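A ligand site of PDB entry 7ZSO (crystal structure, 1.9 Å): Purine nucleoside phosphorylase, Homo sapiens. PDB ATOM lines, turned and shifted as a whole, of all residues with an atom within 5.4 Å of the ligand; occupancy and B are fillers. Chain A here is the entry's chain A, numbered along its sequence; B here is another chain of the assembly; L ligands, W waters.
The backbone NH (N) of Met 219 lies within hydrogen-bond range of the side-chain hydroxyl (OH) of Tyr 192.
NH2 of Arg 84 sits at hydrogen-bond distance from OG1 of Thr 221, 3.0 Å away.
A ring nitrogen (ND1) of His 86 is in hydrogen-bond range of the side-chain hydroxyl of Tyr 88.
NH1 of Arg 84 is in hydrogen-bond range of O of Thr 114 (2.9 Å).
The backbone NH (N) of Gly 32 sits at hydrogen-bond distance from the side-chain hydroxyl (OG1) of Thr 114 (3.0 Å).
The backbone carbonyl oxygen (O) of Val 217 lies within hydrogen-bond range of the backbone NH (N) of Gly 118 (2.8 Å).
The side-chain hydroxyl (OG1) of Thr 221 sits at hydrogen-bond distance from the side-chain hydroxyl (OG) of Ser 220.
O of Leu 240 is in hydrogen-bond range of N of Ala 117 (2.9 Å).
The backbone NH of Ser 33 sits at hydrogen-bond distance from an oxygen (O4) of the ligand (3.0 Å).
N of Ala 116 lies within hydrogen-bond range of O4 of the ligand (3.1 Å).
N of Gly 118 sits close to N2 of the ligand, 3.2 Å away.
OD1 of Asn 243 is in hydrogen-bond range of N2 of the ligand.
NE2 of His 86 sits at hydrogen-bond distance from O3 of the ligand, 2.6 Å away.
An oxygen (O2) of the ligand lies within hydrogen-bond range of the side-chain hydroxyl of Ser 220, 2.6 Å away.
The side-chain hydroxyl (OG) of Ser 33 is in hydrogen-bond range of an oxygen (O4) of the ligand (2.9 Å).
OE2 of Glu 201 lies within hydrogen-bond range of N1 of the ligand (2.6 Å).
The guanidinium group of Arg 84 is in salt-bridge range of an oxygen (O3) of the ligand.
The backbone carbonyl oxygen (O) of Val 260 lies close to a fluorine (F4) of the ligand (2.9 Å).
Merely in contact with the ligand: Gly 32, Gly 34, Asn 115, Ala 117, Phe 200, Val 217, Gly 218, Met 219, Thr 242, Val 245, Leu 261, Gly 264 and Phe 159 of chain B.
Hydrophobic or aromatic side chains that line the ligand: His 86, Ala 116, Phe 200, Val 217, Met 219, Val 245, Val 260, Leu 261 and Phe 159 of chain B.
Of the 33 residues printed, 22 come within 4 Å of the ligand.
Water W2 bridges an oxygen (O5) of the ligand (2.6 Å) and the side-chain carboxylate of Glu 201 (2.8 Å).
Water W3 lies within hydrogen-bond range of O of Ala 116 (2.6 Å), OH of Tyr 192 (2.7 Å), O2 of the ligand (2.8 Å), N of Met 219 (3.1 Å) and OG of Ser 220 (3.3 Å).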
ATOM      1  N   GLY A  32     -22.710  24.075  17.996  1.00  0.00           N
ATOM      2  CA  GLY A  32     -23.551  23.753  19.162  1.00  0.00           C
ATOM      3  C   GLY A  32     -25.036  23.747  18.812  1.00  0.00           C
ATOM      4  O   GLY A  32     -25.409  23.679  17.604  1.00  0.00           O
ATOM      5  N   SER A  33     -25.888  23.846  19.837  1.00  0.00           N
ATOM      6  CA  SER A  33     -27.365  23.801  19.701  1.00  0.00           C
ATOM      7  C   SER A  33     -27.830  24.834  18.671  1.00  0.00           C
ATOM      8  O   SER A  33     -27.436  26.012  18.796  1.00  0.00           O
ATOM      9  CB  SER A  33     -28.002  24.040  21.043  1.00  0.00           C
ATOM     10  OG  SER A  33     -27.538  23.108  21.995  1.00  0.00           O
ATOM     11  N   GLY A  34     -28.641  24.399  17.686  1.00  0.00           N
ATOM     12  CA  GLY A  34     -29.247  25.276  16.677  1.00  0.00           C
ATOM     13  C   GLY A  34     -28.422  25.396  15.405  1.00  0.00           C
ATOM     14  O   GLY A  34     -28.964  25.951  14.423  1.00  0.00           O
ATOM     15  N   ARG A  84     -20.583  18.032  18.933  1.00  0.00           N
ATOM     16  CA  ARG A  84     -19.419  18.020  19.840  1.00  0.00           C
ATOM     17  C   ARG A  84     -19.702  17.067  20.984  1.00  0.00           C
ATOM     18  O   ARG A  84     -20.858  16.778  21.223  1.00  0.00           O
ATOM     19  CB  ARG A  84     -19.200  19.416  20.419  1.00  0.00           C
ATOM     20  CG  ARG A  84     -20.479  20.039  20.965  1.00  0.00           C
ATOM     21  CD  ARG A  84     -20.218  20.674  22.293  1.00  0.00           C
ATOM     22  NE  ARG A  84     -19.396  21.860  22.136  1.00  0.00           N
ATOM     23  CZ  ARG A  84     -19.860  23.063  21.829  1.00  0.00           C
ATOM     24  NH1 ARG A  84     -21.154  23.250  21.629  1.00  0.00           N
ATOM     25  NH2 ARG A  84     -19.035  24.083  21.752  1.00  0.00           N
ATOM     26  N   HIS A  86     -19.718  16.227  25.052  1.00  0.00           N
ATOM     27  CA  HIS A  86     -19.991  16.853  26.364  1.00  0.00           C
ATOM     28  C   HIS A  86     -19.454  15.974  27.481  1.00  0.00           C
ATOM     29  O   HIS A  86     -19.562  14.724  27.388  1.00  0.00           O
ATOM     30  CB  HIS A  86     -21.491  17.123  26.536  1.00  0.00           C
ATOM     31  CG  HIS A  86     -22.081  17.951  25.452  1.00  0.00           C
ATOM     32  ND1 HIS A  86     -22.509  17.406  24.272  1.00  0.00           N
ATOM     33  CD2 HIS A  86     -22.326  19.285  25.375  1.00  0.00           C
ATOM     34  CE1 HIS A  86     -23.011  18.368  23.508  1.00  0.00           C
ATOM     35  NE2 HIS A  86     -22.882  19.514  24.157  1.00  0.00           N
ATOM     36  N   TYR A  88     -21.009  15.665  30.260  1.00  0.00           N
ATOM     37  CA  TYR A  88     -22.200  15.019  30.851  1.00  0.00           C
ATOM     38  C   TYR A  88     -22.467  13.691  30.122  1.00  0.00           C
ATOM     39  O   TYR A  88     -23.185  12.875  30.692  1.00  0.00           O
ATOM     40  CB  TYR A  88     -23.420  15.955  30.869  1.00  0.00           C
ATOM     41  CG  TYR A  88     -23.992  16.356  29.531  1.00  0.00           C
ATOM     42  CD1 TYR A  88     -24.645  15.461  28.708  1.00  0.00           C
ATOM     43  CD2 TYR A  88     -23.889  17.660  29.099  1.00  0.00           C
ATOM     44  CE1 TYR A  88     -25.173  15.851  27.485  1.00  0.00           C
ATOM     45  CE2 TYR A  88     -24.406  18.075  27.888  1.00  0.00           C
ATOM     46  CZ  TYR A  88     -25.056  17.171  27.085  1.00  0.00           C
ATOM     47  OH  TYR A  88     -25.544  17.614  25.895  1.00  0.00           O
ATOM     48  N   THR A 114     -19.924  27.561  19.098  1.00  0.00           N
ATOM     49  CA  THR A 114     -21.256  28.054  19.557  1.00  0.00           C
ATOM     50  C   THR A 114     -21.860  27.082  20.554  1.00  0.00           C
ATOM     51  O   THR A 114     -21.425  25.926  20.618  1.00  0.00           O
ATOM     52  CB  THR A 114     -22.255  28.265  18.418  1.00  0.00           C
ATOM     53  OG1 THR A 114     -22.865  27.029  18.030  1.00  0.00           O
ATOM     54  CG2 THR A 114     -21.593  28.958  17.251  1.00  0.00           C
ATOM     55  N   ASN A 115     -22.836  27.565  21.298  1.00  0.00           N
ATOM     56  CA  ASN A 115     -23.522  26.704  22.276  1.00  0.00           C
ATOM     57  C   ASN A 115     -24.929  27.242  22.515  1.00  0.00           C
ATOM     58  O   ASN A 115     -25.280  28.324  21.961  1.00  0.00           O
ATOM     59  CB  ASN A 115     -22.695  26.539  23.566  1.00  0.00           C
ATOM     60  CG  ASN A 115     -22.438  27.845  24.301  1.00  0.00           C
ATOM     61  OD1 ASN A 115     -23.362  28.603  24.631  1.00  0.00           O
ATOM     62  ND2 ASN A 115     -21.174  28.116  24.574  1.00  0.00           N
ATOM     63  N   ALA A 116     -25.687  26.484  23.309  1.00  0.00           N
ATOM     64  CA  ALA A 116     -26.913  26.949  23.987  1.00  0.00           C
ATOM     65  C   ALA A 116     -26.533  27.230  25.442  1.00  0.00           C
ATOM     66  O   ALA A 116     -25.604  26.595  25.933  1.00  0.00           O
ATOM     67  CB  ALA A 116     -28.007  25.906  23.865  1.00  0.00           C
ATOM     68  N   ALA A 117     -27.207  28.168  26.096  1.00  0.00           N
ATOM     69  CA  ALA A 117     -26.946  28.496  27.519  1.00  0.00           C
ATOM     70  C   ALA A 117     -28.218  29.064  28.158  1.00  0.00           C
ATOM     71  O   ALA A 117     -29.116  29.553  27.409  1.00  0.00           O
ATOM     72  CB  ALA A 117     -25.758  29.424  27.594  1.00  0.00           C
ATOM     73  N   GLY A 118     -28.317  28.967  29.488  1.00  0.00           N
ATOM     74  CA  GLY A 118     -29.383  29.607  30.275  1.00  0.00           C
ATOM     75  C   GLY A 118     -28.977  31.027  30.606  1.00  0.00           C
ATOM     76  O   GLY A 118     -27.811  31.235  30.979  1.00  0.00           O
ATOM     77  N   TYR A 192     -19.714  33.600  30.080  1.00  0.00           N
ATOM     78  CA  TYR A 192     -20.232  32.213  30.114  1.00  0.00           C
ATOM     79  C   TYR A 192     -19.543  31.431  31.232  1.00  0.00           C
ATOM     80  O   TYR A 192     -18.274  31.464  31.309  1.00  0.00           O
ATOM     81  CB  TYR A 192     -19.959  31.573  28.763  1.00  0.00           C
ATOM     82  CG  TYR A 192     -20.365  30.131  28.591  1.00  0.00           C
ATOM     83  CD1 TYR A 192     -19.509  29.104  28.917  1.00  0.00           C
ATOM     84  CD2 TYR A 192     -21.569  29.813  27.989  1.00  0.00           C
ATOM     85  CE1 TYR A 192     -19.840  27.779  28.667  1.00  0.00           C
ATOM     86  CE2 TYR A 192     -21.930  28.487  27.754  1.00  0.00           C
ATOM     87  CZ  TYR A 192     -21.052  27.476  28.075  1.00  0.00           C
ATOM     88  OH  TYR A 192     -21.370  26.179  27.812  1.00  0.00           O
ATOM     89  N   VAL A 195     -20.658  24.640  33.664  1.00  0.00           N
ATOM     90  CA  VAL A 195     -20.986  23.609  34.685  1.00  0.00           C
ATOM     91  C   VAL A 195     -21.063  22.271  33.950  1.00  0.00           C
ATOM     92  O   VAL A 195     -21.326  22.257  32.732  1.00  0.00           O
ATOM     93  CB  VAL A 195     -22.290  23.968  35.422  1.00  0.00           C
ATOM     94  CG1 VAL A 195     -22.176  25.318  36.128  1.00  0.00           C
ATOM     95  CG2 VAL A 195     -23.492  23.949  34.490  1.00  0.00           C
ATOM     96  N   SER A 199     -28.132  17.994  34.746  1.00  0.00           N
ATOM     97  CA  SER A 199     -29.336  18.489  35.458  1.00  0.00           C
ATOM     98  C   SER A 199     -29.300  20.027  35.466  1.00  0.00           C
ATOM     99  O   SER A 199     -28.187  20.623  35.425  1.00  0.00           O
ATOM    100  CB  SER A 199     -29.442  17.865  36.833  1.00  0.00           C
ATOM    101  OG  SER A 199     -28.261  18.061  37.608  1.00  0.00           O
ATOM    102  N   PHE A 200     -30.456  20.679  35.433  1.00  0.00           N
ATOM    103  CA  PHE A 200     -30.544  22.150  35.461  1.00  0.00           C
ATOM    104  C   PHE A 200     -30.375  22.598  36.923  1.00  0.00           C
ATOM    105  O   PHE A 200     -30.608  21.811  37.846  1.00  0.00           O
ATOM    106  CB  PHE A 200     -31.841  22.647  34.828  1.00  0.00           C
ATOM    107  CG  PHE A 200     -31.981  22.465  33.340  1.00  0.00           C
ATOM    108  CD1 PHE A 200     -31.172  23.168  32.452  1.00  0.00           C
ATOM    109  CD2 PHE A 200     -32.945  21.615  32.819  1.00  0.00           C
ATOM    110  CE1 PHE A 200     -31.323  23.027  31.076  1.00  0.00           C
ATOM    111  CE2 PHE A 200     -33.092  21.467  31.438  1.00  0.00           C
ATOM    112  CZ  PHE A 200     -32.272  22.175  30.571  1.00  0.00           C
ATOM    113  N   GLU A 201     -29.965  23.845  37.098  1.00  0.00           N
ATOM    114  CA  GLU A 201     -29.619  24.463  38.402  1.00  0.00           C
ATOM    115  C   GLU A 201     -30.868  24.566  39.284  1.00  0.00           C
ATOM    116  O   GLU A 201     -31.983  24.828  38.767  1.00  0.00           O
ATOM    117  CB  GLU A 201     -29.098  25.894  38.216  1.00  0.00           C
ATOM    118  CG  GLU A 201     -27.724  25.954  37.597  1.00  0.00           C
ATOM    119  CD  GLU A 201     -27.690  25.627  36.121  1.00  0.00           C
ATOM    120  OE1 GLU A 201     -26.745  24.966  35.717  1.00  0.00           O
ATOM    121  OE2 GLU A 201     -28.650  25.996  35.384  1.00  0.00           O
ATOM    122  N   VAL A 217     -25.033  30.392  31.546  1.00  0.00           N
ATOM    123  CA  VAL A 217     -24.499  29.083  32.020  1.00  0.00           C
ATOM    124  C   VAL A 217     -24.790  28.000  30.985  1.00  0.00           C
ATOM    125  O   VAL A 217     -25.932  27.895  30.531  1.00  0.00           O
ATOM    126  CB  VAL A 217     -25.040  28.713  33.419  1.00  0.00           C
ATOM    127  CG1 VAL A 217     -26.566  28.793  33.518  1.00  0.00           C
ATOM    128  CG2 VAL A 217     -24.549  27.347  33.843  1.00  0.00           C
ATOM    129  N   GLY A 218     -23.788  27.173  30.708  1.00  0.00           N
ATOM    130  CA  GLY A 218     -23.935  26.010  29.821  1.00  0.00           C
ATOM    131  C   GLY A 218     -22.963  24.897  30.200  1.00  0.00           C
ATOM    132  O   GLY A 218     -22.291  24.976  31.257  1.00  0.00           O
ATOM    133  N   MET A 219     -22.886  23.881  29.357  1.00  0.00           N
ATOM    134  CA  MET A 219     -22.254  22.602  29.702  1.00  0.00           C
ATOM    135  C   MET A 219     -21.145  22.267  28.697  1.00  0.00           C
ATOM    136  O   MET A 219     -20.774  21.110  28.602  1.00  0.00           O
ATOM    137  CB  MET A 219     -23.316  21.491  29.697  1.00  0.00           C
ATOM    138  CG  MET A 219     -24.481  21.758  30.680  1.00  0.00           C
ATOM    139  SD  MET A 219     -25.807  20.513  30.575  1.00  0.00           S
ATOM    140  CE  MET A 219     -27.040  21.240  31.658  1.00  0.00           C
ATOM    141  N   SER A 220     -20.577  23.253  27.997  1.00  0.00           N
ATOM    142  CA  SER A 220     -19.611  22.961  26.921  1.00  0.00           C
ATOM    143  C   SER A 220     -18.588  24.078  26.739  1.00  0.00           C
ATOM    144  O   SER A 220     -18.521  24.964  27.623  1.00  0.00           O
ATOM    145  CB  SER A 220     -20.345  22.718  25.636  1.00  0.00           C
ATOM    146  OG  SER A 220     -20.881  23.953  25.194  1.00  0.00           O
ATOM    147  N   THR A 221     -17.801  23.991  25.659  1.00  0.00           N
ATOM    148  CA  THR A 221     -17.141  25.143  24.982  1.00  0.00           C
ATOM    149  C   THR A 221     -15.850  25.548  25.687  1.00  0.00           C
ATOM    150  O   THR A 221     -14.849  25.663  25.031  1.00  0.00           O
ATOM    151  CB  THR A 221     -18.088  26.337  24.910  1.00  0.00           C
ATOM    152  OG1 THR A 221     -19.163  25.915  24.067  1.00  0.00           O
ATOM    153  CG2 THR A 221     -17.436  27.588  24.379  1.00  0.00           C
ATOM    154  N   LEU A 240     -26.600  30.818  22.210  1.00  0.00           N
ATOM    155  CA  LEU A 240     -28.060  30.981  22.090  1.00  0.00           C
ATOM    156  C   LEU A 240     -28.659  30.873  23.497  1.00  0.00           C
ATOM    157  O   LEU A 240     -28.494  29.825  24.146  1.00  0.00           O
ATOM    158  CB  LEU A 240     -28.655  29.928  21.157  1.00  0.00           C
ATOM    159  CG  LEU A 240     -30.176  29.989  20.998  1.00  0.00           C
ATOM    160  CD1 LEU A 240     -30.603  31.299  20.348  1.00  0.00           C
ATOM    161  CD2 LEU A 240     -30.692  28.818  20.198  1.00  0.00           C
ATOM    162  N   THR A 242     -31.438  29.918  25.516  1.00  0.00           N
ATOM    163  CA  THR A 242     -32.574  29.007  25.231  1.00  0.00           C
ATOM    164  C   THR A 242     -33.647  29.115  26.319  1.00  0.00           C
ATOM    165  O   THR A 242     -34.702  28.552  26.069  1.00  0.00           O
ATOM    166  CB  THR A 242     -32.086  27.565  25.091  1.00  0.00           C
ATOM    167  OG1 THR A 242     -31.324  27.193  26.240  1.00  0.00           O
ATOM    168  CG2 THR A 242     -31.254  27.358  23.847  1.00  0.00           C
ATOM    169  N   ASN A 243     -33.370  29.741  27.469  1.00  0.00           N
ATOM    170  CA  ASN A 243     -34.220  29.754  28.694  1.00  0.00           C
ATOM    171  C   ASN A 243     -33.607  30.760  29.676  1.00  0.00           C
ATOM    172  O   ASN A 243     -32.411  31.030  29.584  1.00  0.00           O
ATOM    173  CB  ASN A 243     -34.330  28.376  29.359  1.00  0.00           C
ATOM    174  CG  ASN A 243     -32.971  27.817  29.774  1.00  0.00           C
ATOM    175  OD1 ASN A 243     -32.120  27.490  28.923  1.00  0.00           O
ATOM    176  ND2 ASN A 243     -32.747  27.728  31.081  1.00  0.00           N
ATOM    177  N   VAL A 245     -32.768  31.099  33.444  1.00  0.00           N
ATOM    178  CA  VAL A 245     -32.546  30.310  34.682  1.00  0.00           C
ATOM    179  C   VAL A 245     -33.486  30.845  35.767  1.00  0.00           C
ATOM    180  O   VAL A 245     -33.541  32.077  35.933  1.00  0.00           O
ATOM    181  CB  VAL A 245     -31.071  30.411  35.120  1.00  0.00           C
ATOM    182  CG1 VAL A 245     -30.801  29.575  36.350  1.00  0.00           C
ATOM    183  CG2 VAL A 245     -30.124  30.013  33.990  1.00  0.00           C
ATOM    184  N   ALA A 255     -36.981  25.320  34.018  1.00  0.00           N
ATOM    185  CA  ALA A 255     -36.144  24.886  32.871  1.00  0.00           C
ATOM    186  C   ALA A 255     -36.625  23.509  32.427  1.00  0.00           C
ATOM    187  O   ALA A 255     -36.975  22.686  33.304  1.00  0.00           O
ATOM    188  CB  ALA A 255     -34.699  24.836  33.295  1.00  0.00           C
ATOM    189  N   HIS A 257     -36.220  20.360  28.970  1.00  0.00           N
ATOM    190  CA  HIS A 257     -35.658  19.872  27.690  1.00  0.00           C
ATOM    191  C   HIS A 257     -36.527  20.349  26.509  1.00  0.00           C
ATOM    192  O   HIS A 257     -35.976  20.897  25.559  1.00  0.00           O
ATOM    193  CB  HIS A 257     -35.545  18.367  27.778  1.00  0.00           C
ATOM    194  CG  HIS A 257     -34.686  17.774  26.737  1.00  0.00           C
ATOM    195  ND1 HIS A 257     -34.428  16.437  26.706  1.00  0.00           N
ATOM    196  CD2 HIS A 257     -34.029  18.337  25.690  1.00  0.00           C
ATOM    197  CE1 HIS A 257     -33.642  16.177  25.672  1.00  0.00           C
ATOM    198  NE2 HIS A 257     -33.377  17.332  25.040  1.00  0.00           N
ATOM    199  N   VAL A 260     -36.176  24.108  25.642  1.00  0.00           N
ATOM    200  CA  VAL A 260     -34.839  24.510  25.131  1.00  0.00           C
ATOM    201  C   VAL A 260     -34.658  23.907  23.723  1.00  0.00           C
ATOM    202  O   VAL A 260     -34.085  24.602  22.890  1.00  0.00           O
ATOM    203  CB  VAL A 260     -33.656  24.214  26.091  1.00  0.00           C
ATOM    204  CG1 VAL A 260     -33.841  24.877  27.441  1.00  0.00           C
ATOM    205  CG2 VAL A 260     -33.401  22.744  26.288  1.00  0.00           C
ATOM    206  N   LEU A 261     -35.180  22.707  23.438  1.00  0.00           N
ATOM    207  CA  LEU A 261     -35.222  22.161  22.035  1.00  0.00           C
ATOM    208  C   LEU A 261     -36.006  23.122  21.111  1.00  0.00           C
ATOM    209  O   LEU A 261     -35.482  23.479  20.048  1.00  0.00           O
ATOM    210  CB  LEU A 261     -35.871  20.779  22.012  1.00  0.00           C
ATOM    211  CG  LEU A 261     -34.923  19.588  22.101  1.00  0.00           C
ATOM    212  CD1 LEU A 261     -35.711  18.289  22.217  1.00  0.00           C
ATOM    213  CD2 LEU A 261     -33.982  19.517  20.902  1.00  0.00           C
ATOM    214  N   ALA A 263     -36.534  26.289  21.496  1.00  0.00           N
ATOM    215  CA  ALA A 263     -35.750  27.544  21.342  1.00  0.00           C
ATOM    216  C   ALA A 263     -34.659  27.340  20.277  1.00  0.00           C
ATOM    217  O   ALA A 263     -34.445  28.237  19.412  1.00  0.00           O
ATOM    218  CB  ALA A 263     -35.178  27.993  22.656  1.00  0.00           C
ATOM    219  N   GLY A 264     -34.008  26.179  20.309  1.00  0.00           N
ATOM    220  CA  GLY A 264     -32.964  25.870  19.328  1.00  0.00           C
ATOM    221  C   GLY A 264     -33.557  25.801  17.930  1.00  0.00           C
ATOM    222  O   GLY A 264     -32.986  26.393  17.011  1.00  0.00           O
ATOM    223  N   LYS A 265     -34.655  25.072  17.783  1.00  0.00           N
ATOM    224  CA  LYS A 265     -35.337  24.824  16.488  1.00  0.00           C
ATOM    225  C   LYS A 265     -35.783  26.175  15.878  1.00  0.00           C
ATOM    226  O   LYS A 265     -35.489  26.423  14.706  1.00  0.00           O
ATOM    227  CB  LYS A 265     -36.473  23.833  16.745  1.00  0.00           C
ATOM    228  CG  LYS A 265     -36.683  22.775  15.679  1.00  0.00           C
ATOM    229  CD  LYS A 265     -38.033  22.101  15.783  1.00  0.00           C
ATOM    230  CE  LYS A 265     -38.499  21.526  14.470  1.00  0.00           C
ATOM    231  NZ  LYS A 265     -39.937  21.188  14.524  1.00  0.00           N
ATOM    232  N   PHE B 159     -31.909  15.977  30.513  1.00  0.00           N
ATOM    233  CA  PHE B 159     -31.695  17.274  31.224  1.00  0.00           C
ATOM    234  C   PHE B 159     -32.833  17.530  32.207  1.00  0.00           C
ATOM    235  O   PHE B 159     -33.593  18.490  32.049  1.00  0.00           O
ATOM    236  CB  PHE B 159     -31.604  18.482  30.275  1.00  0.00           C
ATOM    237  CG  PHE B 159     -30.635  18.318  29.144  1.00  0.00           C
ATOM    238  CD1 PHE B 159     -29.265  18.347  29.377  1.00  0.00           C
ATOM    239  CD2 PHE B 159     -31.075  18.054  27.857  1.00  0.00           C
ATOM    240  CE1 PHE B 159     -28.360  18.143  28.337  1.00  0.00           C
ATOM    241  CE2 PHE B 159     -30.167  17.873  26.824  1.00  0.00           C
ATOM    242  CZ  PHE B 159     -28.812  17.903  27.064  1.00  0.00           C
HETATM  243  N1  LIG L   1     -28.351  25.645  32.850  1.00  0.00           N
HETATM  244  N2  LIG L   1     -29.649  26.026  29.443  1.00  0.00           N
HETATM  245  C1  LIG L   1     -29.020  25.756  30.626  1.00  0.00           C
HETATM  246  C2  LIG L   1     -27.930  24.701  28.948  1.00  0.00           C
HETATM  247  C3  LIG L   1     -29.009  25.364  28.425  1.00  0.00           C
HETATM  248  C4  LIG L   1     -27.847  22.707  27.077  1.00  0.00           C
HETATM  249  C5  LIG L   1     -27.481  22.284  25.792  1.00  0.00           C
HETATM  250  C6  LIG L   1     -29.622  21.199  25.614  1.00  0.00           C
HETATM  251  C7  LIG L   1     -30.717  21.104  23.616  1.00  0.00           C
HETATM  252  C8  LIG L   1     -31.135  22.928  22.113  1.00  0.00           C
HETATM  253  C9  LIG L   1     -30.856  20.726  21.262  1.00  0.00           C
HETATM  254  C10 LIG L   1     -25.464  21.851  24.365  1.00  0.00           C
HETATM  255  C11 LIG L   1     -29.294  26.141  31.968  1.00  0.00           C
HETATM  256  C12 LIG L   1     -27.313  24.882  32.503  1.00  0.00           C
HETATM  257  N3  LIG L   1     -27.043  24.519  31.287  1.00  0.00           N
HETATM  258  C13 LIG L   1     -27.930  24.935  30.333  1.00  0.00           C
HETATM  259  S1  LIG L   1     -26.780  23.737  28.044  1.00  0.00           S
HETATM  260  C14 LIG L   1     -28.381  21.511  25.060  1.00  0.00           C
HETATM  261  C15 LIG L   1     -29.991  21.650  26.853  1.00  0.00           C
HETATM  262  C16 LIG L   1     -29.089  22.376  27.600  1.00  0.00           C
HETATM  263  O1  LIG L   1     -30.527  20.518  24.835  1.00  0.00           O
HETATM  264  C17 LIG L   1     -30.919  22.450  23.391  1.00  0.00           C
HETATM  265  C18 LIG L   1     -31.086  22.064  21.047  1.00  0.00           C
HETATM  266  C19 LIG L   1     -30.666  20.259  22.540  1.00  0.00           C
HETATM  267  F1  LIG L   1     -30.400  18.965  22.779  1.00  0.00           F
HETATM  268  F2  LIG L   1     -30.810  19.886  20.216  1.00  0.00           F
HETATM  269  F3  LIG L   1     -31.273  22.537  19.803  1.00  0.00           F
HETATM  270  F4  LIG L   1     -31.353  24.241  21.907  1.00  0.00           F
HETATM  271  F5  LIG L   1     -30.988  23.324  24.403  1.00  0.00           F
HETATM  272  C20 LIG L   1     -26.178  22.597  25.208  1.00  0.00           C
HETATM  273  P1  LIG L   1     -24.178  22.642  23.523  1.00  0.00           P
HETATM  274  O2  LIG L   1     -23.351  23.386  24.528  1.00  0.00           O
HETATM  275  O3  LIG L   1     -23.335  21.635  22.753  1.00  0.00           O
HETATM  276  O4  LIG L   1     -24.730  23.652  22.577  1.00  0.00           O
HETATM  277  O5  LIG L   1     -30.231  26.852  32.362  1.00  0.00           O
HETATM  278  O   HOH W   1     -24.205  20.396  20.306  1.00  0.00           O
HETATM  279  O   HOH W   2     -31.347  26.325  34.690  1.00  0.00           O
HETATM  280  O   HOH W   3     -23.556  25.139  26.654  1.00  0.00           O
